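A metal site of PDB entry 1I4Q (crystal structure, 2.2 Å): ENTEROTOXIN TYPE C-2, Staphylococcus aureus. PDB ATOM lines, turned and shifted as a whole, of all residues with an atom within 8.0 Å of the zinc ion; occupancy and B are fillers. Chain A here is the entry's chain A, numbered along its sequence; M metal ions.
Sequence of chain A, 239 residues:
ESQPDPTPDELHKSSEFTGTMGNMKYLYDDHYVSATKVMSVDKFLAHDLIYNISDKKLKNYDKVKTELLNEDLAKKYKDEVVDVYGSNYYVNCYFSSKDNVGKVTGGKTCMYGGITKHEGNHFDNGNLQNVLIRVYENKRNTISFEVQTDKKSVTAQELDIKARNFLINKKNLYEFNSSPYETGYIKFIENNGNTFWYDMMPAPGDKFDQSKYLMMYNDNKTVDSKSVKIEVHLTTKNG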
ATOM      1  N   ALA A  35     -11.160  20.410  -0.573  1.00  0.00           N
ATOM      2  CA  ALA A  35     -10.616  20.014  -1.866  1.00  0.00           C
ATOM      3  C   ALA A  35      -9.145  19.633  -1.774  1.00  0.00           C
ATOM      4  O   ALA A  35      -8.413  20.164  -0.931  1.00  0.00           O
ATOM      5  CB  ALA A  35     -10.793  21.143  -2.873  1.00  0.00           C
ATOM      6  N   THR A  36      -8.715  18.709  -2.620  1.00  0.00           N
ATOM      7  CA  THR A  36      -7.325  18.277  -2.620  1.00  0.00           C
ATOM      8  C   THR A  36      -6.665  18.318  -3.991  1.00  0.00           C
ATOM      9  O   THR A  36      -7.244  17.897  -5.001  1.00  0.00           O
ATOM     10  CB  THR A  36      -7.176  16.836  -2.012  1.00  0.00           C
ATOM     11  OG1 THR A  36      -6.558  15.967  -2.963  1.00  0.00           O
ATOM     12  CG2 THR A  36      -8.517  16.279  -1.598  1.00  0.00           C
ATOM     13  N   LYS A  37      -5.456  18.866  -4.018  1.00  0.00           N
ATOM     14  CA  LYS A  37      -4.658  18.975  -5.238  1.00  0.00           C
ATOM     15  C   LYS A  37      -5.282  19.734  -6.395  1.00  0.00           C
ATOM     16  O   LYS A  37      -5.311  19.245  -7.525  1.00  0.00           O
ATOM     17  CB  LYS A  37      -4.243  17.568  -5.693  1.00  0.00           C
ATOM     18  CG  LYS A  37      -3.271  16.881  -4.741  1.00  0.00           C
ATOM     19  CD  LYS A  37      -3.008  15.432  -5.129  1.00  0.00           C
ATOM     20  CE  LYS A  37      -2.364  15.328  -6.506  1.00  0.00           C
ATOM     21  NZ  LYS A  37      -2.109  13.903  -6.862  1.00  0.00           N
ATOM     22  N   VAL A  38      -5.778  20.934  -6.112  1.00  0.00           N
ATOM     23  CA  VAL A  38      -6.381  21.770  -7.149  1.00  0.00           C
ATOM     24  C   VAL A  38      -5.461  22.968  -7.443  1.00  0.00           C
ATOM     25  O   VAL A  38      -4.539  23.264  -6.675  1.00  0.00           O
ATOM     26  CB  VAL A  38      -7.779  22.286  -6.710  1.00  0.00           C
ATOM     27  CG1 VAL A  38      -8.798  21.142  -6.735  1.00  0.00           C
ATOM     28  CG2 VAL A  38      -7.708  22.882  -5.314  1.00  0.00           C
ATOM     29  N   VAL A  81      -0.208  23.697  -6.673  1.00  0.00           N
ATOM     30  CA  VAL A  81      -1.154  22.605  -6.515  1.00  0.00           C
ATOM     31  C   VAL A  81      -1.404  22.603  -5.002  1.00  0.00           C
ATOM     32  O   VAL A  81      -0.504  22.270  -4.230  1.00  0.00           O
ATOM     33  CB  VAL A  81      -0.553  21.242  -6.953  1.00  0.00           C
ATOM     34  CG1 VAL A  81      -1.486  20.109  -6.565  1.00  0.00           C
ATOM     35  CG2 VAL A  81      -0.313  21.237  -8.459  1.00  0.00           C
ATOM     36  N   VAL A  82      -2.601  22.997  -4.594  1.00  0.00           N
ATOM     37  CA  VAL A  82      -2.925  23.094  -3.176  1.00  0.00           C
ATOM     38  C   VAL A  82      -4.126  22.274  -2.721  1.00  0.00           C
ATOM     39  O   VAL A  82      -4.863  21.704  -3.519  1.00  0.00           O
ATOM     40  CB  VAL A  82      -3.223  24.562  -2.775  1.00  0.00           C
ATOM     41  CG1 VAL A  82      -2.043  25.457  -3.103  1.00  0.00           C
ATOM     42  CG2 VAL A  82      -4.460  25.049  -3.517  1.00  0.00           C
ATOM     43  N   ASP A  83      -4.298  22.245  -1.394  1.00  0.00           N
ATOM     44  CA  ASP A  83      -5.426  21.584  -0.757  1.00  0.00           C
ATOM     45  C   ASP A  83      -6.183  22.758  -0.153  1.00  0.00           C
ATOM     46  O   ASP A  83      -5.567  23.751   0.254  1.00  0.00           O
ATOM     47  CB  ASP A  83      -4.973  20.645   0.375  1.00  0.00           C
ATOM     48  CG  ASP A  83      -4.128  19.489  -0.112  1.00  0.00           C
ATOM     49  OD1 ASP A  83      -4.490  18.877  -1.144  1.00  0.00           O
ATOM     50  OD2 ASP A  83      -3.107  19.191   0.544  1.00  0.00           O
ATOM     51  N   VAL A  84      -7.500  22.646  -0.096  1.00  0.00           N
ATOM     52  CA  VAL A  84      -8.353  23.711   0.419  1.00  0.00           C
ATOM     53  C   VAL A  84      -9.274  23.249   1.549  1.00  0.00           C
ATOM     54  O   VAL A  84      -9.787  22.131   1.533  1.00  0.00           O
ATOM     55  CB  VAL A  84      -9.238  24.287  -0.724  1.00  0.00           C
ATOM     56  CG1 VAL A  84     -10.135  25.399  -0.215  1.00  0.00           C
ATOM     57  CG2 VAL A  84      -8.346  24.767  -1.869  1.00  0.00           C
ATOM     58  N   THR A 116      -3.326  25.533   1.396  1.00  0.00           N
ATOM     59  CA  THR A 116      -1.997  25.038   1.759  1.00  0.00           C
ATOM     60  C   THR A 116      -1.466  24.193   0.608  1.00  0.00           C
ATOM     61  O   THR A 116      -2.215  23.479  -0.050  1.00  0.00           O
ATOM     62  CB  THR A 116      -2.054  24.158   3.019  1.00  0.00           C
ATOM     63  OG1 THR A 116      -3.098  23.185   2.874  1.00  0.00           O
ATOM     64  CG2 THR A 116      -2.305  24.998   4.260  1.00  0.00           C
ATOM     65  N   LYS A 117      -0.163  24.259   0.378  1.00  0.00           N
ATOM     66  CA  LYS A 117       0.449  23.476  -0.697  1.00  0.00           C
ATOM     67  C   LYS A 117       0.261  22.013  -0.355  1.00  0.00           C
ATOM     68  O   LYS A 117       0.326  21.632   0.816  1.00  0.00           O
ATOM     69  CB  LYS A 117       1.939  23.798  -0.796  1.00  0.00           C
ATOM     70  CG  LYS A 117       2.215  25.277  -0.905  1.00  0.00           C
ATOM     71  CD  LYS A 117       3.682  25.607  -0.670  1.00  0.00           C
ATOM     72  CE  LYS A 117       3.898  27.106  -0.742  1.00  0.00           C
ATOM     73  NZ  LYS A 117       5.299  27.500  -0.459  1.00  0.00           N
ATOM     74  N   HIS A 118       0.018  21.190  -1.368  1.00  0.00           N
ATOM     75  CA  HIS A 118      -0.170  19.771  -1.159  1.00  0.00           C
ATOM     76  C   HIS A 118       1.152  19.057  -0.918  1.00  0.00           C
ATOM     77  O   HIS A 118       1.323  18.333   0.077  1.00  0.00           O
ATOM     78  CB  HIS A 118      -0.842  19.151  -2.388  1.00  0.00           C
ATOM     79  CG  HIS A 118      -0.704  17.665  -2.465  1.00  0.00           C
ATOM     80  ND1 HIS A 118      -1.292  16.808  -1.556  1.00  0.00           N
ATOM     81  CD2 HIS A 118      -0.037  16.878  -3.341  1.00  0.00           C
ATOM     82  CE1 HIS A 118      -0.990  15.555  -1.866  1.00  0.00           C
ATOM     83  NE2 HIS A 118      -0.229  15.568  -2.947  1.00  0.00           N
ATOM     84  N   GLU A 119       2.081  19.262  -1.846  1.00  0.00           N
ATOM     85  CA  GLU A 119       3.400  18.629  -1.799  1.00  0.00           C
ATOM     86  C   GLU A 119       4.136  18.829  -0.473  1.00  0.00           C
ATOM     87  O   GLU A 119       4.242  19.953   0.020  1.00  0.00           O
ATOM     88  CB  GLU A 119       4.252  19.140  -2.961  1.00  0.00           C
ATOM     89  CG  GLU A 119       5.268  18.147  -3.515  1.00  0.00           C
ATOM     90  CD  GLU A 119       4.623  16.911  -4.132  1.00  0.00           C
ATOM     91  OE1 GLU A 119       4.051  16.091  -3.375  1.00  0.00           O
ATOM     92  OE2 GLU A 119       4.684  16.761  -5.373  1.00  0.00           O
ATOM     93  N   GLY A 120       4.629  17.731   0.080  1.00  0.00           N
ATOM     94  CA  GLY A 120       5.376  17.760   1.328  1.00  0.00           C
ATOM     95  C   GLY A 120       4.649  18.202   2.589  1.00  0.00           C
ATOM     96  O   GLY A 120       5.281  18.491   3.598  1.00  0.00           O
ATOM     97  N   ASN A 121       3.316  18.235   2.545  1.00  0.00           N
ATOM     98  CA  ASN A 121       2.557  18.672   3.706  1.00  0.00           C
ATOM     99  C   ASN A 121       1.755  17.573   4.413  1.00  0.00           C
ATOM    100  O   ASN A 121       0.829  17.879   5.170  1.00  0.00           O
ATOM    101  CB  ASN A 121       1.621  19.821   3.309  1.00  0.00           C
ATOM    102  CG  ASN A 121       1.077  20.572   4.523  1.00  0.00           C
ATOM    103  OD1 ASN A 121       1.836  20.953   5.412  1.00  0.00           O
ATOM    104  ND2 ASN A 121      -0.235  20.778   4.548  1.00  0.00           N
ATOM    105  N   HIS A 122       2.095  16.315   4.169  1.00  0.00           N
ATOM    106  CA  HIS A 122       1.389  15.202   4.809  1.00  0.00           C
ATOM    107  C   HIS A 122       2.353  14.298   5.589  1.00  0.00           C
ATOM    108  O   HIS A 122       3.568  14.368   5.392  1.00  0.00           O
ATOM    109  CB  HIS A 122       0.620  14.399   3.757  1.00  0.00           C
ATOM    110  CG  HIS A 122      -0.528  15.157   3.162  1.00  0.00           C
ATOM    111  ND1 HIS A 122      -1.600  15.601   3.916  1.00  0.00           N
ATOM    112  CD2 HIS A 122      -0.772  15.571   1.897  1.00  0.00           C
ATOM    113  CE1 HIS A 122      -2.438  16.252   3.144  1.00  0.00           C
ATOM    114  NE2 HIS A 122      -1.964  16.249   1.914  1.00  0.00           N
ATOM    115  N   ASP A 150      -4.929  15.883   8.378  1.00  0.00           N
ATOM    116  CA  ASP A 150      -3.960  15.090   7.647  1.00  0.00           C
ATOM    117  C   ASP A 150      -2.804  15.977   7.178  1.00  0.00           C
ATOM    118  O   ASP A 150      -1.946  15.537   6.419  1.00  0.00           O
ATOM    119  CB  ASP A 150      -4.633  14.464   6.426  1.00  0.00           C
ATOM    120  CG  ASP A 150      -5.020  15.502   5.385  1.00  0.00           C
ATOM    121  OD1 ASP A 150      -5.485  16.593   5.778  1.00  0.00           O
ATOM    122  OD2 ASP A 150      -4.881  15.225   4.178  1.00  0.00           O
ATOM    123  N   LYS A 151      -2.805  17.225   7.633  1.00  0.00           N
ATOM    124  CA  LYS A 151      -1.759  18.173   7.231  1.00  0.00           C
ATOM    125  C   LYS A 151      -0.757  18.479   8.333  1.00  0.00           C
ATOM    126  O   LYS A 151      -1.121  18.627   9.500  1.00  0.00           O
ATOM    127  CB  LYS A 151      -2.391  19.482   6.764  1.00  0.00           C
ATOM    128  CG  LYS A 151      -3.380  19.337   5.616  1.00  0.00           C
ATOM    129  CD  LYS A 151      -3.958  20.693   5.221  1.00  0.00           C
ATOM    130  CE  LYS A 151      -5.075  20.564   4.206  1.00  0.00           C
ATOM    131  NZ  LYS A 151      -6.284  19.905   4.784  1.00  0.00           N
HETATM  132 ZN    ZN M   1      -2.701  17.200   0.105  1.00  0.00          ZN
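The side-chain carboxylate (OD1) of Asp 83 is in hydrogen-bond range of the backbone NH (N) of Lys 37 (3.0 Å). The backbone carbonyl oxygen (O) of Thr 116 is in hydrogen-bond range of the backbone NH (N) of Asp 83 (2.8 Å). The backbone carbonyl oxygen (O) of Asp 150 is in hydrogen-bond range of a ring nitrogen (ND1) of His 122, 2.5 Å away. The backbone NH of His 118 is in hydrogen-bond range of the backbone carbonyl oxygen of Val 81, at 3.1 Å.
Three residues have an atom within 4 Å of the zinc ion: Asp 83, His 118 and His 122.
The zinc ion is bound by OD2 of Asp 83 (2.1 Å), NE2 of His 122 (2.2 Å) and ND1 of His 118 (2.2 Å). The zinc ion has three donor atoms within binding distance. Slightly farther from the zinc ion lies OD1 of Asp 83 (2.8 Å).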
